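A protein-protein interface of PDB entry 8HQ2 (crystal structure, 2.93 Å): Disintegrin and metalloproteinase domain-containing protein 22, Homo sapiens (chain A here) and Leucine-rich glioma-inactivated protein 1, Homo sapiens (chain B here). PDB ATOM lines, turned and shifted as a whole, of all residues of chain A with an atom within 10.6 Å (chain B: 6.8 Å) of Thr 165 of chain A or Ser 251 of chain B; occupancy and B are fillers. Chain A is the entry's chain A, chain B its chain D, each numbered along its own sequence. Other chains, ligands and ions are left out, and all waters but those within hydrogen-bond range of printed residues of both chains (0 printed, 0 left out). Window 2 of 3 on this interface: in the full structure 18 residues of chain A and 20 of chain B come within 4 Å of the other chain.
CZ of Phe 272 of chain B touches CE of Lys 161 of chain A, 3.6 Å away.
CB of Thr 165 of chain A touches CD2 of Phe 272 of chain B, 3.5 Å away.
Trp 166 of chain A touches Pro 224 of chain B (CH2 to CB, 3.5 Å).
Trp 166 of chain A touches Ser 251 of chain B (CE3 to CB, 3.8 Å).
Trp 166 of chain A touches Val 253 of chain B (CH2 to CG2, 3.6 Å).
CD2 of Leu 271 of chain B touches O of Trp 166 of chain A, at 3.2 Å.
Asp 173 of chain A touches Lys 300 of chain B (O to CE, 3.6 Å).
CA of Gly 175 of chain A touches CB of Lys 300 of chain B (3.6 Å).
The side-chain hydroxyl (OG1) of Thr 165 of chain A lies within hydrogen-bond range of the side-chain hydroxyl (OG) of Ser 251 of chain B.
Of the 17 printed residues of chain A, 5 touch a printed residue of chain B.
Among the printed residues, 9 pairs touch across the chains.
The backbone carbonyl oxygen of Ala 269 of chain B lies within hydrogen-bond range of the backbone NH of Val 253 of chain B, at 2.8 Å.
The side-chain carboxylate (OD1) of Asp 164 of chain A lies within hydrogen-bond range of the backbone NH (N) of Trp 166 of chain A.
The backbone carbonyl oxygen (O) of Ser 251 of chain B lies within hydrogen-bond range of the backbone NH (N) of Leu 271 of chain B (2.9 Å).
SG of Cys 162 of chain A is disulfide-bonded to SG of Cys 169 of chain A.
Of chain B, only Ser 251 (3.0 Å) and Phe 272 (3.5 Å) come within 4 Å of Thr 165 of chain A.
Ser 251 of chain B touches just these residues of chain A: Thr 165 and Trp 166.
No residue of chain A comes within 4 Å of Gly 227 of chain B.
Gly 249 of chain B touches none of the printed residues of chain A.
No residue of chain A comes within 4 Å of Thr 250 of chain B.
No residue of chain A comes within 4 Å of Thr 252 of chain B.
Phe 272 of chain B touches just these residues of chain A: Lys 161 and Thr 165.
Printed residues of chain B within 4 Å of Trp 166 of chain A: Pro 224 (3.5 Å), Ser 251 (3.8 Å), Val 253 (3.6 Å) and Leu 271 (3.2 Å).
Of the printed residues of chain B, Asp 173 of chain A touches Lys 300.
Of the printed residues of chain B, Gly 175 of chain A touches Lys 300.
Of the printed residues of chain B, Lys 161 of chain A touches Phe 272.
Printed residues of chain A within 4 Å of Val 253 of chain B: Trp 166 (3.6 Å).
The nearest residue of chain B that does not touch Thr 165 of chain A is Leu 271 of chain B (4.2 Å).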
ATOM      1  N   LYS A 161      25.363  11.100   1.152  1.00  0.00           N
ATOM      2  CA  LYS A 161      24.939  11.497   2.486  1.00  0.00           C
ATOM      3  C   LYS A 161      25.114  12.998   2.635  1.00  0.00           C
ATOM      4  O   LYS A 161      26.155  13.541   2.252  1.00  0.00           O
ATOM      5  CB  LYS A 161      25.741  10.760   3.566  1.00  0.00           C
ATOM      6  CG  LYS A 161      25.638  11.389   4.947  1.00  0.00           C
ATOM      7  CD  LYS A 161      26.769  10.943   5.858  1.00  0.00           C
ATOM      8  CE  LYS A 161      26.764  11.727   7.162  1.00  0.00           C
ATOM      9  NZ  LYS A 161      27.804  11.229   8.104  1.00  0.00           N
ATOM     10  N   CYS A 162      24.104  13.661   3.189  1.00  0.00           N
ATOM     11  CA  CYS A 162      24.251  15.065   3.544  1.00  0.00           C
ATOM     12  C   CYS A 162      25.214  15.162   4.721  1.00  0.00           C
ATOM     13  O   CYS A 162      25.001  14.525   5.759  1.00  0.00           O
ATOM     14  CB  CYS A 162      22.890  15.669   3.890  1.00  0.00           C
ATOM     15  SG  CYS A 162      22.887  17.448   4.255  1.00  0.00           S
ATOM     16  N   GLU A 163      26.288  15.928   4.553  1.00  0.00           N
ATOM     17  CA  GLU A 163      27.331  15.970   5.569  1.00  0.00           C
ATOM     18  C   GLU A 163      27.026  16.958   6.688  1.00  0.00           C
ATOM     19  O   GLU A 163      27.840  17.098   7.607  1.00  0.00           O
ATOM     20  CB  GLU A 163      28.684  16.303   4.930  1.00  0.00           C
ATOM     21  CG  GLU A 163      28.685  17.539   4.051  1.00  0.00           C
ATOM     22  CD  GLU A 163      30.076  17.904   3.570  1.00  0.00           C
ATOM     23  OE1 GLU A 163      30.998  17.080   3.742  1.00  0.00           O
ATOM     24  OE2 GLU A 163      30.252  19.016   3.030  1.00  0.00           O
ATOM     25  N   ASP A 164      25.884  17.636   6.637  1.00  0.00           N
ATOM     26  CA  ASP A 164      25.448  18.504   7.724  1.00  0.00           C
ATOM     27  C   ASP A 164      24.558  17.679   8.646  1.00  0.00           C
ATOM     28  O   ASP A 164      23.457  17.275   8.263  1.00  0.00           O
ATOM     29  CB  ASP A 164      24.716  19.728   7.176  1.00  0.00           C
ATOM     30  CG  ASP A 164      24.427  20.775   8.244  1.00  0.00           C
ATOM     31  OD1 ASP A 164      24.170  20.405   9.409  1.00  0.00           O
ATOM     32  OD2 ASP A 164      24.458  21.981   7.917  1.00  0.00           O
ATOM     33  N   THR A 165      25.045  17.415   9.859  1.00  0.00           N
ATOM     34  CA  THR A 165      24.301  16.573  10.789  1.00  0.00           C
ATOM     35  C   THR A 165      23.193  17.348  11.497  1.00  0.00           C
ATOM     36  O   THR A 165      22.098  16.811  11.710  1.00  0.00           O
ATOM     37  CB  THR A 165      25.252  15.954  11.812  1.00  0.00           C
ATOM     38  OG1 THR A 165      25.606  16.938  12.791  1.00  0.00           O
ATOM     39  CG2 THR A 165      26.514  15.459  11.129  1.00  0.00           C
ATOM     40  N   TRP A 166      23.454  18.600  11.880  1.00  0.00           N
ATOM     41  CA  TRP A 166      22.473  19.363  12.646  1.00  0.00           C
ATOM     42  C   TRP A 166      21.234  19.667  11.813  1.00  0.00           C
ATOM     43  O   TRP A 166      20.120  19.264  12.163  1.00  0.00           O
ATOM     44  CB  TRP A 166      23.109  20.655  13.161  1.00  0.00           C
ATOM     45  CG  TRP A 166      22.210  21.436  14.059  1.00  0.00           C
ATOM     46  CD1 TRP A 166      21.594  22.618  13.775  1.00  0.00           C
ATOM     47  CD2 TRP A 166      21.807  21.080  15.384  1.00  0.00           C
ATOM     48  NE1 TRP A 166      20.840  23.028  14.848  1.00  0.00           N
ATOM     49  CE2 TRP A 166      20.953  22.099  15.848  1.00  0.00           C
ATOM     50  CE3 TRP A 166      22.089  20.001  16.226  1.00  0.00           C
ATOM     51  CZ2 TRP A 166      20.380  22.071  17.116  1.00  0.00           C
ATOM     52  CZ3 TRP A 166      21.519  19.973  17.484  1.00  0.00           C
ATOM     53  CH2 TRP A 166      20.675  21.001  17.918  1.00  0.00           C
ATOM     54  N   SER A 167      21.408  20.355  10.696  1.00  0.00           N
ATOM     55  CA  SER A 167      20.334  20.589   9.746  1.00  0.00           C
ATOM     56  C   SER A 167      20.583  19.709   8.530  1.00  0.00           C
ATOM     57  O   SER A 167      21.734  19.479   8.148  1.00  0.00           O
ATOM     58  CB  SER A 167      20.263  22.066   9.344  1.00  0.00           C
ATOM     59  OG  SER A 167      21.528  22.527   8.896  1.00  0.00           O
ATOM     60  N   GLY A 168      19.510  19.207   7.930  1.00  0.00           N
ATOM     61  CA  GLY A 168      19.646  18.332   6.783  1.00  0.00           C
ATOM     62  C   GLY A 168      20.097  19.067   5.538  1.00  0.00           C
ATOM     63  O   GLY A 168      20.642  20.172   5.632  1.00  0.00           O
ATOM     64  N   CYS A 169      19.941  18.440   4.381  1.00  0.00           N
ATOM     65  CA  CYS A 169      20.036  19.136   3.110  1.00  0.00           C
ATOM     66  C   CYS A 169      18.621  19.424   2.607  1.00  0.00           C
ATOM     67  O   CYS A 169      17.633  19.066   3.249  1.00  0.00           O
ATOM     68  CB  CYS A 169      20.862  18.325   2.108  1.00  0.00           C
ATOM     69  SG  CYS A 169      22.653  18.351   2.445  1.00  0.00           S
ATOM     70  N   ASP A 173      14.132  15.435   4.893  1.00  0.00           N
ATOM     71  CA  ASP A 173      13.059  15.885   5.773  1.00  0.00           C
ATOM     72  C   ASP A 173      13.468  17.173   6.478  1.00  0.00           C
ATOM     73  O   ASP A 173      14.577  17.279   7.011  1.00  0.00           O
ATOM     74  CB  ASP A 173      12.721  14.807   6.804  1.00  0.00           C
ATOM     75  CG  ASP A 173      12.360  13.481   6.166  1.00  0.00           C
ATOM     76  OD1 ASP A 173      11.773  13.485   5.063  1.00  0.00           O
ATOM     77  OD2 ASP A 173      12.654  12.430   6.777  1.00  0.00           O
ATOM     78  N   GLY A 175      13.131  19.778   9.421  1.00  0.00           N
ATOM     79  CA  GLY A 175      12.720  20.040  10.784  1.00  0.00           C
ATOM     80  C   GLY A 175      12.642  21.527  11.057  1.00  0.00           C
ATOM     81  O   GLY A 175      12.536  22.350  10.144  1.00  0.00           O
ATOM     82  N   TYR A 177      15.061  23.363  12.192  1.00  0.00           N
ATOM     83  CA  TYR A 177      16.295  23.963  11.698  1.00  0.00           C
ATOM     84  C   TYR A 177      16.411  23.678  10.203  1.00  0.00           C
ATOM     85  O   TYR A 177      16.462  22.514   9.788  1.00  0.00           O
ATOM     86  CB  TYR A 177      17.499  23.420  12.464  1.00  0.00           C
ATOM     87  CG  TYR A 177      17.434  23.689  13.952  1.00  0.00           C
ATOM     88  CD1 TYR A 177      17.851  24.905  14.480  1.00  0.00           C
ATOM     89  CD2 TYR A 177      16.951  22.726  14.832  1.00  0.00           C
ATOM     90  CE1 TYR A 177      17.794  25.151  15.839  1.00  0.00           C
ATOM     91  CE2 TYR A 177      16.889  22.966  16.194  1.00  0.00           C
ATOM     92  CZ  TYR A 177      17.312  24.179  16.690  1.00  0.00           C
ATOM     93  OH  TYR A 177      17.252  24.420  18.044  1.00  0.00           O
ATOM     94  N   LEU A 178      16.449  24.753   9.388  1.00  0.00           N
ATOM     95  CA  LEU A 178      16.259  24.646   7.947  1.00  0.00           C
ATOM     96  C   LEU A 178      17.589  24.456   7.222  1.00  0.00           C
ATOM     97  O   LEU A 178      18.598  25.060   7.602  1.00  0.00           O
ATOM     98  CB  LEU A 178      15.556  25.889   7.412  1.00  0.00           C
ATOM     99  CG  LEU A 178      14.159  26.067   8.001  1.00  0.00           C
ATOM    100  CD1 LEU A 178      13.466  27.247   7.371  1.00  0.00           C
ATOM    101  CD2 LEU A 178      13.337  24.800   7.820  1.00  0.00           C
ATOM    102  N   PRO A 179      17.597  23.592   6.206  1.00  0.00           N
ATOM    103  CA  PRO A 179      18.800  23.402   5.385  1.00  0.00           C
ATOM    104  C   PRO A 179      19.015  24.537   4.394  1.00  0.00           C
ATOM    105  O   PRO A 179      18.067  25.052   3.796  1.00  0.00           O
ATOM    106  CB  PRO A 179      18.514  22.087   4.658  1.00  0.00           C
ATOM    107  CG  PRO A 179      17.026  22.042   4.554  1.00  0.00           C
ATOM    108  CD  PRO A 179      16.487  22.719   5.784  1.00  0.00           C
ATOM    109  N   LYS A 180      20.273  24.965   4.257  1.00  0.00           N
ATOM    110  CA  LYS A 180      20.662  25.889   3.198  1.00  0.00           C
ATOM    111  C   LYS A 180      21.476  25.276   2.060  1.00  0.00           C
ATOM    112  O   LYS A 180      21.780  25.989   1.098  1.00  0.00           O
ATOM    113  CB  LYS A 180      21.424  27.075   3.798  1.00  0.00           C
ATOM    114  CG  LYS A 180      20.685  28.403   3.647  1.00  0.00           C
ATOM    115  CD  LYS A 180      19.238  28.297   4.125  1.00  0.00           C
ATOM    116  CE  LYS A 180      18.456  29.573   3.839  1.00  0.00           C
ATOM    117  NZ  LYS A 180      17.001  29.428   4.144  1.00  0.00           N
ATOM    118  N   LYS A 181      21.850  23.994   2.127  1.00  0.00           N
ATOM    119  CA  LYS A 181      22.835  23.450   1.195  1.00  0.00           C
ATOM    120  C   LYS A 181      22.377  22.138   0.569  1.00  0.00           C
ATOM    121  O   LYS A 181      21.779  21.290   1.238  1.00  0.00           O
ATOM    122  CB  LYS A 181      24.194  23.235   1.879  1.00  0.00           C
ATOM    123  CG  LYS A 181      24.995  24.515   2.057  1.00  0.00           C
ATOM    124  CD  LYS A 181      26.446  24.236   2.415  1.00  0.00           C
ATOM    125  CE  LYS A 181      27.224  25.537   2.561  1.00  0.00           C
ATOM    126  NZ  LYS A 181      27.065  26.429   1.374  1.00  0.00           N
ATOM    127  N   THR A 183      23.205  18.471  -1.320  1.00  0.00           N
ATOM    128  CA  THR A 183      24.203  17.409  -1.342  1.00  0.00           C
ATOM    129  C   THR A 183      24.993  17.455  -2.647  1.00  0.00           C
ATOM    130  O   THR A 183      24.514  17.956  -3.668  1.00  0.00           O
ATOM    131  CB  THR A 183      23.529  16.038  -1.199  1.00  0.00           C
ATOM    132  OG1 THR A 183      22.556  16.082  -0.149  1.00  0.00           O
ATOM    133  CG2 THR A 183      24.550  14.958  -0.884  1.00  0.00           C
ATOM    134  N   GLN B 223      24.261  19.485  25.107  1.00  0.00           N
ATOM    135  CA  GLN B 223      25.159  20.297  24.303  1.00  0.00           C
ATOM    136  C   GLN B 223      24.994  19.908  22.844  1.00  0.00           C
ATOM    137  O   GLN B 223      25.344  18.778  22.472  1.00  0.00           O
ATOM    138  CB  GLN B 223      26.607  20.119  24.745  1.00  0.00           C
ATOM    139  CG  GLN B 223      27.567  20.986  23.957  1.00  0.00           C
ATOM    140  CD  GLN B 223      28.955  20.991  24.542  1.00  0.00           C
ATOM    141  OE1 GLN B 223      29.213  20.351  25.561  1.00  0.00           O
ATOM    142  NE2 GLN B 223      29.865  21.705  23.894  1.00  0.00           N
ATOM    143  N   PRO B 224      24.479  20.792  21.988  1.00  0.00           N
ATOM    144  CA  PRO B 224      24.136  20.360  20.623  1.00  0.00           C
ATOM    145  C   PRO B 224      25.334  20.005  19.755  1.00  0.00           C
ATOM    146  O   PRO B 224      25.288  19.001  19.036  1.00  0.00           O
ATOM    147  CB  PRO B 224      23.371  21.571  20.067  1.00  0.00           C
ATOM    148  CG  PRO B 224      23.930  22.742  20.825  1.00  0.00           C
ATOM    149  CD  PRO B 224      24.228  22.228  22.206  1.00  0.00           C
ATOM    150  N   PHE B 225      26.408  20.795  19.803  1.00  0.00           N
ATOM    151  CA  PHE B 225      27.441  20.722  18.775  1.00  0.00           C
ATOM    152  C   PHE B 225      28.527  19.689  19.050  1.00  0.00           C
ATOM    153  O   PHE B 225      29.252  19.321  18.117  1.00  0.00           O
ATOM    154  CB  PHE B 225      28.065  22.101  18.578  1.00  0.00           C
ATOM    155  CG  PHE B 225      27.068  23.151  18.197  1.00  0.00           C
ATOM    156  CD1 PHE B 225      26.437  23.102  16.965  1.00  0.00           C
ATOM    157  CD2 PHE B 225      26.739  24.169  19.076  1.00  0.00           C
ATOM    158  CE1 PHE B 225      25.507  24.056  16.609  1.00  0.00           C
ATOM    159  CE2 PHE B 225      25.810  25.129  18.725  1.00  0.00           C
ATOM    160  CZ  PHE B 225      25.193  25.073  17.491  1.00  0.00           C
ATOM    161  N   THR B 226      28.676  19.223  20.290  1.00  0.00           N
ATOM    162  CA  THR B 226      29.491  18.046  20.562  1.00  0.00           C
ATOM    163  C   THR B 226      28.670  16.764  20.610  1.00  0.00           C
ATOM    164  O   THR B 226      29.251  15.674  20.655  1.00  0.00           O
ATOM    165  CB  THR B 226      30.262  18.207  21.880  1.00  0.00           C
ATOM    166  OG1 THR B 226      31.249  17.173  21.987  1.00  0.00           O
ATOM    167  CG2 THR B 226      29.329  18.090  23.050  1.00  0.00           C
ATOM    168  N   GLY B 227      27.342  16.870  20.595  1.00  0.00           N
ATOM    169  CA  GLY B 227      26.480  15.716  20.714  1.00  0.00           C
ATOM    170  C   GLY B 227      26.425  15.093  22.090  1.00  0.00           C
ATOM    171  O   GLY B 227      25.705  14.106  22.273  1.00  0.00           O
ATOM    172  N   LYS B 228      27.148  15.632  23.065  1.00  0.00           N
ATOM    173  CA  LYS B 228      27.176  15.037  24.389  1.00  0.00           C
ATOM    174  C   LYS B 228      25.965  15.465  25.204  1.00  0.00           C
ATOM    175  O   LYS B 228      25.441  16.573  25.060  1.00  0.00           O
ATOM    176  CB  LYS B 228      28.454  15.417  25.135  1.00  0.00           C
ATOM    177  CG  LYS B 228      29.723  14.856  24.517  1.00  0.00           C
ATOM    178  CD  LYS B 228      30.955  15.416  25.200  1.00  0.00           C
ATOM    179  CE  LYS B 228      32.239  15.027  24.481  1.00  0.00           C
ATOM    180  NZ  LYS B 228      32.464  13.555  24.464  1.00  0.00           N
ATOM    181  N   GLY B 249      26.277  11.173  22.127  1.00  0.00           N
ATOM    182  CA  GLY B 249      25.340  11.083  21.029  1.00  0.00           C
ATOM    183  C   GLY B 249      25.779  12.034  19.936  1.00  0.00           C
ATOM    184  O   GLY B 249      26.837  12.659  20.024  1.00  0.00           O
ATOM    185  N   THR B 250      24.965  12.132  18.889  1.00  0.00           N
ATOM    186  CA  THR B 250      25.242  13.029  17.773  1.00  0.00           C
ATOM    187  C   THR B 250      24.057  13.961  17.588  1.00  0.00           C
ATOM    188  O   THR B 250      22.925  13.500  17.408  1.00  0.00           O
ATOM    189  CB  THR B 250      25.518  12.256  16.481  1.00  0.00           C
ATOM    190  OG1 THR B 250      26.666  11.418  16.658  1.00  0.00           O
ATOM    191  CG2 THR B 250      25.780  13.221  15.333  1.00  0.00           C
ATOM    192  N   SER B 251      24.320  15.267  17.630  1.00  0.00           N
ATOM    193  CA  SER B 251      23.283  16.283  17.467  1.00  0.00           C
ATOM    194  C   SER B 251      22.181  16.114  18.509  1.00  0.00           C
ATOM    195  O   SER B 251      20.994  16.038  18.188  1.00  0.00           O
ATOM    196  CB  SER B 251      22.713  16.260  16.047  1.00  0.00           C
ATOM    197  OG  SER B 251      23.742  16.449  15.094  1.00  0.00           O
ATOM    198  N   THR B 252      22.588  16.037  19.773  1.00  0.00           N
ATOM    199  CA  THR B 252      21.617  15.941  20.856  1.00  0.00           C
ATOM    200  C   THR B 252      20.892  17.271  21.050  1.00  0.00           C
ATOM    201  O   THR B 252      21.519  18.328  21.200  1.00  0.00           O
ATOM    202  CB  THR B 252      22.297  15.520  22.159  1.00  0.00           C
ATOM    203  OG1 THR B 252      23.561  16.178  22.279  1.00  0.00           O
ATOM    204  CG2 THR B 252      22.494  14.008  22.205  1.00  0.00           C
ATOM    205  N   VAL B 253      19.558  17.197  21.076  1.00  0.00           N
ATOM    206  CA  VAL B 253      18.680  18.354  21.245  1.00  0.00           C
ATOM    207  C   VAL B 253      18.135  18.428  22.674  1.00  0.00           C
ATOM    208  O   VAL B 253      18.379  19.408  23.386  1.00  0.00           O
ATOM    209  CB  VAL B 253      17.543  18.355  20.194  1.00  0.00           C
ATOM    210  CG1 VAL B 253      16.435  19.316  20.590  1.00  0.00           C
ATOM    211  CG2 VAL B 253      18.094  18.725  18.848  1.00  0.00           C
ATOM    212  N   VAL B 254      17.353  17.439  23.086  1.00  0.00           N
ATOM    213  CA  VAL B 254      16.735  17.425  24.406  1.00  0.00           C
ATOM    214  C   VAL B 254      17.242  16.208  25.173  1.00  0.00           C
ATOM    215  O   VAL B 254      17.310  15.106  24.621  1.00  0.00           O
ATOM    216  CB  VAL B 254      15.193  17.422  24.316  1.00  0.00           C
ATOM    217  CG1 VAL B 254      14.564  17.355  25.707  1.00  0.00           C
ATOM    218  CG2 VAL B 254      14.695  18.658  23.591  1.00  0.00           C
ATOM    219  N   ALA B 269      16.968  12.960  22.792  1.00  0.00           N
ATOM    220  CA  ALA B 269      16.538  13.122  21.415  1.00  0.00           C
ATOM    221  C   ALA B 269      17.686  13.694  20.598  1.00  0.00           C
ATOM    222  O   ALA B 269      18.327  14.664  21.016  1.00  0.00           O
ATOM    223  CB  ALA B 269      15.317  14.040  21.337  1.00  0.00           C
ATOM    224  N   GLN B 270      17.950  13.090  19.444  1.00  0.00           N
ATOM    225  CA  GLN B 270      19.008  13.548  18.560  1.00  0.00           C
ATOM    226  C   GLN B 270      18.435  13.808  17.177  1.00  0.00           C
ATOM    227  O   GLN B 270      17.376  13.293  16.810  1.00  0.00           O
ATOM    228  CB  GLN B 270      20.151  12.532  18.465  1.00  0.00           C
ATOM    229  CG  GLN B 270      20.407  11.761  19.742  1.00  0.00           C
ATOM    230  CD  GLN B 270      21.589  10.827  19.622  1.00  0.00           C
ATOM    231  OE1 GLN B 270      22.700  11.256  19.318  1.00  0.00           O
ATOM    232  NE2 GLN B 270      21.357   9.542  19.853  1.00  0.00           N
ATOM    233  N   LEU B 271      19.147  14.630  16.412  1.00  0.00           N
ATOM    234  CA  LEU B 271      18.778  14.892  15.029  1.00  0.00           C
ATOM    235  C   LEU B 271      19.397  13.905  14.046  1.00  0.00           C
ATOM    236  O   LEU B 271      18.965  13.860  12.890  1.00  0.00           O
ATOM    237  CB  LEU B 271      19.169  16.325  14.648  1.00  0.00           C
ATOM    238  CG  LEU B 271      18.078  17.397  14.778  1.00  0.00           C
ATOM    239  CD1 LEU B 271      17.097  17.076  15.894  1.00  0.00           C
ATOM    240  CD2 LEU B 271      18.688  18.771  14.991  1.00  0.00           C
ATOM    241  N   PHE B 272      20.394  13.122  14.469  1.00  0.00           N
ATOM    242  CA  PHE B 272      21.041  12.128  13.616  1.00  0.00           C
ATOM    243  C   PHE B 272      20.800  10.738  14.194  1.00  0.00           C
ATOM    244  O   PHE B 272      21.454  10.348  15.166  1.00  0.00           O
ATOM    245  CB  PHE B 272      22.539  12.414  13.510  1.00  0.00           C
ATOM    246  CG  PHE B 272      23.123  12.102  12.166  1.00  0.00           C
ATOM    247  CD1 PHE B 272      23.561  10.824  11.863  1.00  0.00           C
ATOM    248  CD2 PHE B 272      23.241  13.092  11.207  1.00  0.00           C
ATOM    249  CE1 PHE B 272      24.101  10.541  10.624  1.00  0.00           C
ATOM    250  CE2 PHE B 272      23.780  12.817   9.970  1.00  0.00           C
ATOM    251  CZ  PHE B 272      24.209  11.540   9.677  1.00  0.00           C
ATOM    252  N   LYS B 300      12.728  14.747  13.398  1.00  0.00           N
ATOM    253  CA  LYS B 300      13.414  15.963  13.832  1.00  0.00           C
ATOM    254  C   LYS B 300      12.796  16.433  15.148  1.00  0.00           C
ATOM    255  O   LYS B 300      12.030  17.410  15.173  1.00  0.00           O
ATOM    256  CB  LYS B 300      13.333  17.050  12.762  1.00  0.00           C
ATOM    257  CG  LYS B 300      13.908  16.646  11.414  1.00  0.00           C
ATOM    258  CD  LYS B 300      15.419  16.479  11.477  1.00  0.00           C
ATOM    259  CE  LYS B 300      15.993  16.073  10.126  1.00  0.00           C
ATOM    260  NZ  LYS B 300      17.479  16.167  10.117  1.00  0.00           N
